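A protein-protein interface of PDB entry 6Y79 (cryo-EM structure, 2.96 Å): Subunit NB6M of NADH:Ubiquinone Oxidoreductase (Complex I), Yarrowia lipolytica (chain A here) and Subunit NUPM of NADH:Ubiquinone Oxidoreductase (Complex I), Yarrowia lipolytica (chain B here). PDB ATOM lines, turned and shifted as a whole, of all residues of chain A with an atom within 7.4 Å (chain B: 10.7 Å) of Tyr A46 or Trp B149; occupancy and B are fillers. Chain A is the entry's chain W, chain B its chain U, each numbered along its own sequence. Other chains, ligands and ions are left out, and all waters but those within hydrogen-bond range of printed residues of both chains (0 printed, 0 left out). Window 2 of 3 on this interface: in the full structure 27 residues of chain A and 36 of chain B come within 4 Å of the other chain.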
ATOM      1  N   ILE A  40       6.523  22.867 -25.528  1.00  0.00           N
ATOM      2  CA  ILE A  40       6.014  24.225 -25.719  1.00  0.00           C
ATOM      3  C   ILE A  40       4.931  24.247 -26.791  1.00  0.00           C
ATOM      4  O   ILE A  40       3.859  24.837 -26.600  1.00  0.00           O
ATOM      5  CB  ILE A  40       7.169  25.180 -26.075  1.00  0.00           C
ATOM      6  CG1 ILE A  40       8.127  25.367 -24.894  1.00  0.00           C
ATOM      7  CG2 ILE A  40       6.649  26.530 -26.543  1.00  0.00           C
ATOM      8  CD1 ILE A  40       7.469  25.798 -23.615  1.00  0.00           C
ATOM      9  N   CYS A  41       5.182  23.578 -27.921  1.00  0.00           N
ATOM     10  CA  CYS A  41       4.230  23.578 -29.026  1.00  0.00           C
ATOM     11  C   CYS A  41       2.954  22.828 -28.667  1.00  0.00           C
ATOM     12  O   CYS A  41       1.852  23.259 -29.023  1.00  0.00           O
ATOM     13  CB  CYS A  41       4.875  22.980 -30.279  1.00  0.00           C
ATOM     14  SG  CYS A  41       6.176  23.987 -31.031  1.00  0.00           S
ATOM     15  N   GLY A  42       3.074  21.716 -27.932  1.00  0.00           N
ATOM     16  CA  GLY A  42       1.891  20.978 -27.532  1.00  0.00           C
ATOM     17  C   GLY A  42       1.046  21.713 -26.517  1.00  0.00           C
ATOM     18  O   GLY A  42      -0.185  21.649 -26.570  1.00  0.00           O
ATOM     19  N   TYR A  43       1.684  22.446 -25.602  1.00  0.00           N
ATOM     20  CA  TYR A  43       0.922  23.267 -24.669  1.00  0.00           C
ATOM     21  C   TYR A  43       0.223  24.420 -25.381  1.00  0.00           C
ATOM     22  O   TYR A  43      -0.913  24.785 -25.032  1.00  0.00           O
ATOM     23  CB  TYR A  43       1.840  23.798 -23.581  1.00  0.00           C
ATOM     24  CG  TYR A  43       1.104  24.618 -22.577  1.00  0.00           C
ATOM     25  CD1 TYR A  43       0.225  24.021 -21.690  1.00  0.00           C
ATOM     26  CD2 TYR A  43       1.271  25.990 -22.522  1.00  0.00           C
ATOM     27  CE1 TYR A  43      -0.463  24.767 -20.771  1.00  0.00           C
ATOM     28  CE2 TYR A  43       0.591  26.746 -21.607  1.00  0.00           C
ATOM     29  CZ  TYR A  43      -0.276  26.130 -20.736  1.00  0.00           C
ATOM     30  OH  TYR A  43      -0.960  26.886 -19.818  1.00  0.00           O
ATOM     31  N   GLY A  44       0.881  24.999 -26.386  1.00  0.00           N
ATOM     32  CA  GLY A  44       0.228  26.021 -27.183  1.00  0.00           C
ATOM     33  C   GLY A  44      -0.952  25.487 -27.969  1.00  0.00           C
ATOM     34  O   GLY A  44      -1.966  26.169 -28.115  1.00  0.00           O
ATOM     35  N   PHE A  45      -0.839  24.259 -28.483  1.00  0.00           N
ATOM     36  CA  PHE A  45      -1.962  23.641 -29.184  1.00  0.00           C
ATOM     37  C   PHE A  45      -3.107  23.339 -28.232  1.00  0.00           C
ATOM     38  O   PHE A  45      -4.276  23.433 -28.618  1.00  0.00           O
ATOM     39  CB  PHE A  45      -1.519  22.363 -29.884  1.00  0.00           C
ATOM     40  CG  PHE A  45      -1.104  22.565 -31.301  1.00  0.00           C
ATOM     41  CD1 PHE A  45      -2.046  22.742 -32.295  1.00  0.00           C
ATOM     42  CD2 PHE A  45       0.235  22.565 -31.644  1.00  0.00           C
ATOM     43  CE1 PHE A  45      -1.659  22.924 -33.605  1.00  0.00           C
ATOM     44  CE2 PHE A  45       0.628  22.749 -32.946  1.00  0.00           C
ATOM     45  CZ  PHE A  45      -0.319  22.929 -33.928  1.00  0.00           C
ATOM     46  N   TYR A  46      -2.778  22.962 -26.991  1.00  0.00           N
ATOM     47  CA  TYR A  46      -3.777  22.786 -25.941  1.00  0.00           C
ATOM     48  C   TYR A  46      -4.603  24.049 -25.745  1.00  0.00           C
ATOM     49  O   TYR A  46      -5.839  24.018 -25.836  1.00  0.00           O
ATOM     50  CB  TYR A  46      -3.084  22.382 -24.639  1.00  0.00           C
ATOM     51  CG  TYR A  46      -3.967  22.357 -23.416  1.00  0.00           C
ATOM     52  CD1 TYR A  46      -4.759  21.263 -23.145  1.00  0.00           C
ATOM     53  CD2 TYR A  46      -3.982  23.413 -22.514  1.00  0.00           C
ATOM     54  CE1 TYR A  46      -5.567  21.226 -22.031  1.00  0.00           C
ATOM     55  CE2 TYR A  46      -4.786  23.385 -21.400  1.00  0.00           C
ATOM     56  CZ  TYR A  46      -5.576  22.290 -21.164  1.00  0.00           C
ATOM     57  OH  TYR A  46      -6.378  22.251 -20.050  1.00  0.00           O
ATOM     58  N   ARG A  47      -3.923  25.177 -25.525  1.00  0.00           N
ATOM     59  CA  ARG A  47      -4.632  26.435 -25.296  1.00  0.00           C
ATOM     60  C   ARG A  47      -5.382  26.910 -26.534  1.00  0.00           C
ATOM     61  O   ARG A  47      -6.504  27.415 -26.426  1.00  0.00           O
ATOM     62  CB  ARG A  47      -3.658  27.506 -24.837  1.00  0.00           C
ATOM     63  CG  ARG A  47      -3.077  27.241 -23.491  1.00  0.00           C
ATOM     64  CD  ARG A  47      -2.227  28.405 -23.085  1.00  0.00           C
ATOM     65  NE  ARG A  47      -3.020  29.618 -22.962  1.00  0.00           N
ATOM     66  CZ  ARG A  47      -3.603  30.009 -21.837  1.00  0.00           C
ATOM     67  NH1 ARG A  47      -4.310  31.125 -21.808  1.00  0.00           N
ATOM     68  NH2 ARG A  47      -3.478  29.285 -20.738  1.00  0.00           N
ATOM     69  N   ALA A  48      -4.795  26.728 -27.719  1.00  0.00           N
ATOM     70  CA  ALA A  48      -5.415  27.203 -28.952  1.00  0.00           C
ATOM     71  C   ALA A  48      -6.678  26.421 -29.284  1.00  0.00           C
ATOM     72  O   ALA A  48      -7.710  27.012 -29.623  1.00  0.00           O
ATOM     73  CB  ALA A  48      -4.417  27.111 -30.103  1.00  0.00           C
ATOM     74  N   LEU A  49      -6.621  25.092 -29.185  1.00  0.00           N
ATOM     75  CA  LEU A  49      -7.785  24.282 -29.510  1.00  0.00           C
ATOM     76  C   LEU A  49      -8.868  24.421 -28.451  1.00  0.00           C
ATOM     77  O   LEU A  49     -10.063  24.413 -28.790  1.00  0.00           O
ATOM     78  CB  LEU A  49      -7.369  22.824 -29.695  1.00  0.00           C
ATOM     79  CG  LEU A  49      -7.063  22.392 -31.135  1.00  0.00           C
ATOM     80  CD1 LEU A  49      -5.849  23.085 -31.714  1.00  0.00           C
ATOM     81  CD2 LEU A  49      -6.867  20.902 -31.214  1.00  0.00           C
ATOM     82  N   GLY A  50      -8.472  24.613 -27.185  1.00  0.00           N
ATOM     83  CA  GLY A  50      -9.445  24.969 -26.167  1.00  0.00           C
ATOM     84  C   GLY A  50     -10.165  26.267 -26.473  1.00  0.00           C
ATOM     85  O   GLY A  50     -11.397  26.322 -26.421  1.00  0.00           O
ATOM     86  N   GLY A  51      -9.415  27.298 -26.876  1.00  0.00           N
ATOM     87  CA  GLY A  51     -10.023  28.573 -27.219  1.00  0.00           C
ATOM     88  C   GLY A  51     -10.922  28.530 -28.439  1.00  0.00           C
ATOM     89  O   GLY A  51     -11.937  29.232 -28.478  1.00  0.00           O
ATOM     90  N   ILE A  52     -10.586  27.698 -29.431  1.00  0.00           N
ATOM     91  CA  ILE A  52     -11.465  27.533 -30.589  1.00  0.00           C
ATOM     92  C   ILE A  52     -12.778  26.878 -30.176  1.00  0.00           C
ATOM     93  O   ILE A  52     -13.858  27.282 -30.637  1.00  0.00           O
ATOM     94  CB  ILE A  52     -10.772  26.728 -31.704  1.00  0.00           C
ATOM     95  CG1 ILE A  52      -9.570  27.465 -32.264  1.00  0.00           C
ATOM     96  CG2 ILE A  52     -11.705  26.482 -32.864  1.00  0.00           C
ATOM     97  CD1 ILE A  52      -8.735  26.608 -33.169  1.00  0.00           C
ATOM     98  N   GLN A  53     -12.721  25.883 -29.283  1.00  0.00           N
ATOM     99  CA  GLN A  53     -13.962  25.246 -28.841  1.00  0.00           C
ATOM    100  C   GLN A  53     -14.842  26.201 -28.032  1.00  0.00           C
ATOM    101  O   GLN A  53     -16.074  26.202 -28.197  1.00  0.00           O
ATOM    102  CB  GLN A  53     -13.646  23.979 -28.058  1.00  0.00           C
ATOM    103  CG  GLN A  53     -13.031  22.911 -28.927  1.00  0.00           C
ATOM    104  CD  GLN A  53     -12.569  21.718 -28.148  1.00  0.00           C
ATOM    105  OE1 GLN A  53     -13.089  21.430 -27.078  1.00  0.00           O
ATOM    106  NE2 GLN A  53     -11.576  21.018 -28.672  1.00  0.00           N
ATOM    107  N   GLU A  54     -14.228  27.061 -27.207  1.00  0.00           N
ATOM    108  CA  GLU A  54     -14.997  28.080 -26.485  1.00  0.00           C
ATOM    109  C   GLU A  54     -15.639  29.065 -27.428  1.00  0.00           C
ATOM    110  O   GLU A  54     -16.761  29.521 -27.197  1.00  0.00           O
ATOM    111  CB  GLU A  54     -14.107  28.875 -25.557  1.00  0.00           C
ATOM    112  CG  GLU A  54     -13.447  28.052 -24.587  1.00  0.00           C
ATOM    113  CD  GLU A  54     -14.339  27.592 -23.534  1.00  0.00           C
ATOM    114  OE1 GLU A  54     -15.270  28.338 -23.131  1.00  0.00           O
ATOM    115  OE2 GLU A  54     -14.156  26.435 -23.049  1.00  0.00           O
ATOM    116  N   ARG A  55     -14.889  29.486 -28.434  1.00  0.00           N
ATOM    117  CA  ARG A  55     -15.405  30.456 -29.376  1.00  0.00           C
ATOM    118  C   ARG A  55     -16.558  29.877 -30.183  1.00  0.00           C
ATOM    119  O   ARG A  55     -17.509  30.594 -30.508  1.00  0.00           O
ATOM    120  CB  ARG A  55     -14.262  30.908 -30.266  1.00  0.00           C
ATOM    121  CG  ARG A  55     -14.563  32.071 -31.100  1.00  0.00           C
ATOM    122  CD  ARG A  55     -13.286  32.573 -31.706  1.00  0.00           C
ATOM    123  NE  ARG A  55     -12.742  31.678 -32.724  1.00  0.00           N
ATOM    124  CZ  ARG A  55     -11.598  31.020 -32.596  1.00  0.00           C
ATOM    125  NH1 ARG A  55     -10.891  31.137 -31.482  1.00  0.00           N
ATOM    126  NH2 ARG A  55     -11.166  30.242 -33.576  1.00  0.00           N
ATOM    127  N   SER B 109     -19.715  37.733 -24.776  1.00  0.00           N
ATOM    128  CA  SER B 109     -18.589  37.140 -24.069  1.00  0.00           C
ATOM    129  C   SER B 109     -17.984  38.081 -23.043  1.00  0.00           C
ATOM    130  O   SER B 109     -17.330  37.615 -22.107  1.00  0.00           O
ATOM    131  CB  SER B 109     -17.511  36.734 -25.067  1.00  0.00           C
ATOM    132  OG  SER B 109     -16.942  37.880 -25.675  1.00  0.00           O
ATOM    133  N   GLY B 110     -18.173  39.385 -23.200  1.00  0.00           N
ATOM    134  CA  GLY B 110     -17.528  40.364 -22.359  1.00  0.00           C
ATOM    135  C   GLY B 110     -18.392  41.016 -21.308  1.00  0.00           C
ATOM    136  O   GLY B 110     -18.007  42.060 -20.778  1.00  0.00           O
ATOM    137  N   ARG B 112     -20.240  39.203 -18.572  1.00  0.00           N
ATOM    138  CA  ARG B 112     -20.736  38.082 -17.781  1.00  0.00           C
ATOM    139  C   ARG B 112     -21.198  38.515 -16.395  1.00  0.00           C
ATOM    140  O   ARG B 112     -22.205  38.009 -15.885  1.00  0.00           O
ATOM    141  CB  ARG B 112     -19.656  37.013 -17.677  1.00  0.00           C
ATOM    142  CG  ARG B 112     -19.310  36.397 -19.006  1.00  0.00           C
ATOM    143  CD  ARG B 112     -20.517  35.693 -19.580  1.00  0.00           C
ATOM    144  NE  ARG B 112     -20.167  34.885 -20.740  1.00  0.00           N
ATOM    145  CZ  ARG B 112     -21.009  34.582 -21.718  1.00  0.00           C
ATOM    146  NH1 ARG B 112     -20.604  33.844 -22.731  1.00  0.00           N
ATOM    147  NH2 ARG B 112     -22.257  35.022 -21.686  1.00  0.00           N
ATOM    148  N   GLU B 140     -21.825  21.704 -20.731  1.00  0.00           N
ATOM    149  CA  GLU B 140     -22.093  22.880 -19.901  1.00  0.00           C
ATOM    150  C   GLU B 140     -22.500  24.066 -20.776  1.00  0.00           C
ATOM    151  O   GLU B 140     -21.930  24.258 -21.856  1.00  0.00           O
ATOM    152  CB  GLU B 140     -20.870  23.240 -19.041  1.00  0.00           C
ATOM    153  CG  GLU B 140     -19.558  23.434 -19.798  1.00  0.00           C
ATOM    154  CD  GLU B 140     -18.418  23.857 -18.892  1.00  0.00           C
ATOM    155  OE1 GLU B 140     -18.653  24.024 -17.680  1.00  0.00           O
ATOM    156  OE2 GLU B 140     -17.288  24.030 -19.393  1.00  0.00           O
ATOM    157  N   VAL B 142     -22.434  27.941 -21.872  1.00  0.00           N
ATOM    158  CA  VAL B 142     -21.257  28.805 -21.884  1.00  0.00           C
ATOM    159  C   VAL B 142     -21.321  29.929 -20.848  1.00  0.00           C
ATOM    160  O   VAL B 142     -20.299  30.275 -20.245  1.00  0.00           O
ATOM    161  CB  VAL B 142     -21.045  29.345 -23.316  1.00  0.00           C
ATOM    162  CG1 VAL B 142     -22.268  30.108 -23.841  1.00  0.00           C
ATOM    163  CG2 VAL B 142     -19.769  30.187 -23.418  1.00  0.00           C
ATOM    164  N   PHE B 143     -22.496  30.472 -20.570  1.00  0.00           N
ATOM    165  CA  PHE B 143     -22.642  31.581 -19.635  1.00  0.00           C
ATOM    166  C   PHE B 143     -22.774  31.119 -18.187  1.00  0.00           C
ATOM    167  O   PHE B 143     -23.166  31.911 -17.327  1.00  0.00           O
ATOM    168  CB  PHE B 143     -23.832  32.462 -20.047  1.00  0.00           C
ATOM    169  CG  PHE B 143     -25.170  31.759 -20.032  1.00  0.00           C
ATOM    170  CD1 PHE B 143     -25.558  30.918 -21.070  1.00  0.00           C
ATOM    171  CD2 PHE B 143     -26.069  31.996 -19.010  1.00  0.00           C
ATOM    172  CE1 PHE B 143     -26.780  30.293 -21.055  1.00  0.00           C
ATOM    173  CE2 PHE B 143     -27.305  31.383 -19.002  1.00  0.00           C
ATOM    174  CZ  PHE B 143     -27.655  30.526 -20.024  1.00  0.00           C
ATOM    175  N   LEU B 144     -22.448  29.855 -17.911  1.00  0.00           N
ATOM    176  CA  LEU B 144     -22.429  29.298 -16.570  1.00  0.00           C
ATOM    177  C   LEU B 144     -21.037  28.909 -16.107  1.00  0.00           C
ATOM    178  O   LEU B 144     -20.844  28.682 -14.908  1.00  0.00           O
ATOM    179  CB  LEU B 144     -23.317  28.049 -16.490  1.00  0.00           C
ATOM    180  CG  LEU B 144     -24.815  28.115 -16.190  1.00  0.00           C
ATOM    181  CD1 LEU B 144     -25.059  28.769 -14.847  1.00  0.00           C
ATOM    182  CD2 LEU B 144     -25.583  28.814 -17.270  1.00  0.00           C
ATOM    183  N   LYS B 145     -20.076  28.816 -17.014  1.00  0.00           N
ATOM    184  CA  LYS B 145     -18.810  28.187 -16.693  1.00  0.00           C
ATOM    185  C   LYS B 145     -17.900  29.123 -15.911  1.00  0.00           C
ATOM    186  O   LYS B 145     -17.978  30.350 -16.020  1.00  0.00           O
ATOM    187  CB  LYS B 145     -18.116  27.724 -17.964  1.00  0.00           C
ATOM    188  CG  LYS B 145     -17.705  28.817 -18.910  1.00  0.00           C
ATOM    189  CD  LYS B 145     -17.033  28.156 -20.088  1.00  0.00           C
ATOM    190  CE  LYS B 145     -15.757  27.481 -19.607  1.00  0.00           C
ATOM    191  NZ  LYS B 145     -15.150  26.555 -20.604  1.00  0.00           N
ATOM    192  N   LYS B 146     -17.034  28.518 -15.107  1.00  0.00           N
ATOM    193  CA  LYS B 146     -16.110  29.236 -14.246  1.00  0.00           C
ATOM    194  C   LYS B 146     -14.716  29.201 -14.855  1.00  0.00           C
ATOM    195  O   LYS B 146     -14.236  28.140 -15.267  1.00  0.00           O
ATOM    196  CB  LYS B 146     -16.088  28.633 -12.840  1.00  0.00           C
ATOM    197  CG  LYS B 146     -17.245  29.062 -11.951  1.00  0.00           C
ATOM    198  CD  LYS B 146     -18.456  28.160 -12.114  1.00  0.00           C
ATOM    199  CE  LYS B 146     -19.663  28.717 -11.380  1.00  0.00           C
ATOM    200  NZ  LYS B 146     -20.932  28.148 -11.907  1.00  0.00           N
ATOM    201  N   ASP B 147     -14.071  30.371 -14.885  1.00  0.00           N
ATOM    202  CA  ASP B 147     -12.842  30.671 -15.614  1.00  0.00           C
ATOM    203  C   ASP B 147     -12.947  30.264 -17.078  1.00  0.00           C
ATOM    204  O   ASP B 147     -12.402  29.225 -17.467  1.00  0.00           O
ATOM    205  CB  ASP B 147     -11.627  30.001 -14.971  1.00  0.00           C
ATOM    206  CG  ASP B 147     -11.181  30.700 -13.707  1.00  0.00           C
ATOM    207  OD1 ASP B 147     -10.894  31.915 -13.767  1.00  0.00           O
ATOM    208  OD2 ASP B 147     -11.112  30.032 -12.655  1.00  0.00           O
ATOM    209  N   PRO B 148     -13.660  31.024 -17.906  1.00  0.00           N
ATOM    210  CA  PRO B 148     -13.628  30.762 -19.344  1.00  0.00           C
ATOM    211  C   PRO B 148     -12.284  31.156 -19.928  1.00  0.00           C
ATOM    212  O   PRO B 148     -11.531  31.941 -19.353  1.00  0.00           O
ATOM    213  CB  PRO B 148     -14.749  31.649 -19.896  1.00  0.00           C
ATOM    214  CG  PRO B 148     -15.528  32.082 -18.700  1.00  0.00           C
ATOM    215  CD  PRO B 148     -14.529  32.170 -17.610  1.00  0.00           C
ATOM    216  N   TRP B 149     -11.982  30.575 -21.085  1.00  0.00           N
ATOM    217  CA  TRP B 149     -10.748  30.911 -21.777  1.00  0.00           C
ATOM    218  C   TRP B 149     -10.799  32.326 -22.327  1.00  0.00           C
ATOM    219  O   TRP B 149      -9.773  33.010 -22.405  1.00  0.00           O
ATOM    220  CB  TRP B 149     -10.509  29.917 -22.904  1.00  0.00           C
ATOM    221  CG  TRP B 149     -10.197  28.514 -22.466  1.00  0.00           C
ATOM    222  CD1 TRP B 149     -11.110  27.521 -22.216  1.00  0.00           C
ATOM    223  CD2 TRP B 149      -8.914  27.922 -22.298  1.00  0.00           C
ATOM    224  NE1 TRP B 149     -10.481  26.366 -21.879  1.00  0.00           N
ATOM    225  CE2 TRP B 149      -9.124  26.580 -21.922  1.00  0.00           C
ATOM    226  CE3 TRP B 149      -7.614  28.392 -22.410  1.00  0.00           C
ATOM    227  CZ2 TRP B 149      -8.072  25.718 -21.660  1.00  0.00           C
ATOM    228  CZ3 TRP B 149      -6.580  27.536 -22.154  1.00  0.00           C
ATOM    229  CH2 TRP B 149      -6.804  26.220 -21.783  1.00  0.00           C
ATOM    230  N   ILE B 150     -11.986  32.786 -22.698  1.00  0.00           N
ATOM    231  CA  ILE B 150     -12.165  34.057 -23.385  1.00  0.00           C
ATOM    232  C   ILE B 150     -12.796  35.030 -22.405  1.00  0.00           C
ATOM    233  O   ILE B 150     -14.010  35.005 -22.169  1.00  0.00           O
ATOM    234  CB  ILE B 150     -13.011  33.900 -24.654  1.00  0.00           C
ATOM    235  CG1 ILE B 150     -12.313  32.925 -25.598  1.00  0.00           C
ATOM    236  CG2 ILE B 150     -13.217  35.237 -25.341  1.00  0.00           C
ATOM    237  CD1 ILE B 150     -13.082  32.622 -26.829  1.00  0.00           C
ATOM    238  N   LYS B 151     -12.007  35.828 -21.855  1.00  0.00           N
ATOM    239  CA  LYS B 151     -12.238  36.974 -21.011  1.00  0.00           C
ATOM    240  C   LYS B 151     -12.192  38.239 -21.854  1.00  0.00           C
ATOM    241  O   LYS B 151     -11.517  38.273 -22.886  1.00  0.00           O
ATOM    242  CB  LYS B 151     -11.173  37.048 -19.916  1.00  0.00           C
ATOM    243  CG  LYS B 151     -11.137  35.830 -19.026  1.00  0.00           C
ATOM    244  CD  LYS B 151     -10.087  35.971 -17.952  1.00  0.00           C
ATOM    245  CE  LYS B 151     -10.141  34.806 -16.988  1.00  0.00           C
ATOM    246  NZ  LYS B 151      -9.096  34.917 -15.933  1.00  0.00           N
ATOM    247  N   PRO B 152     -12.909  39.291 -21.486  1.00  0.00           N
ATOM    248  CA  PRO B 152     -12.826  40.538 -22.244  1.00  0.00           C
ATOM    249  C   PRO B 152     -11.552  41.305 -21.921  1.00  0.00           C
ATOM    250  O   PRO B 152     -10.754  40.921 -21.067  1.00  0.00           O
ATOM    251  CB  PRO B 152     -14.064  41.309 -21.798  1.00  0.00           C
ATOM    252  CG  PRO B 152     -14.392  40.760 -20.494  1.00  0.00           C
ATOM    253  CD  PRO B 152     -14.007  39.323 -20.510  1.00  0.00           C
ATOM    254  N   ALA B 153     -11.376  42.407 -22.649  1.00  0.00           N
ATOM    255  CA  ALA B 153     -10.191  43.237 -22.479  1.00  0.00           C
ATOM    256  C   ALA B 153     -10.206  43.939 -21.132  1.00  0.00           C
ATOM    257  O   ALA B 153      -9.289  43.770 -20.323  1.00  0.00           O
ATOM    258  CB  ALA B 153     -10.103  44.255 -23.611  1.00  0.00           C
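Among the printed residues, pairs that only touch across the chains: Glu A54 with Trp B149 (3.3 Å), Tyr A46 with Trp B149 (3.5 Å), Arg A47 with Trp B149 (3.8 Å), Gly A51 with Ile B150 (3.9 Å) and Arg A55 with Ile B150 (3.96 Å).
The side-chain carboxylate (OE2) of Glu A54 is in salt-bridge range of the side-chain amino group (NZ) of Lys B145 (2.6 Å).
No residue of chain B comes within 4 Å of Gly A42. Tyr A43 touches none of the printed residues of chain B. Tyr A46 touches just one residue of chain B: Trp B149 (3.5 Å). Arg A47 touches just one residue of chain B: Trp B149 (3.8 Å). No residue of chain B comes within 4 Å of Ala A48. Leu A49 touches none of the printed residues of chain B. Of the printed residues of chain B, Arg A55 touches Ile B150 (3.96 Å). Printed residues of chain A within 4 Å of Lys B145: Glu A54 (2.6 Å). Pro B148 touches none of the printed residues of chain A. Trp B149 touches just these residues of chain A: Tyr A46 (3.5 Å), Arg A47 (3.8 Å) and Glu A54 (3.3 Å). The nearest residue of chain A that does not touch Trp B149 is Gly A50 (4.4 Å).
The side-chain amino group of Lys B145 lies within salt-bridge range of the side-chain carboxylate of Glu B140 (3.5 Å).
Printed residues of chain A that touch a printed residue of chain B: Tyr A46, Arg A47, Gly A51, Glu A54 and Arg A55. Of the 16 printed residues of chain B, 3 touch a printed residue of chain A. Hydrophobic or aromatic side chains of chain B within 4 Å of the printed part of chain A: Trp B149 and Ile B150. Along chain B the printed residues that touch a printed residue of chain A span positions 145 to 150. Among the printed residues, 6 pairs touch across the chains.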
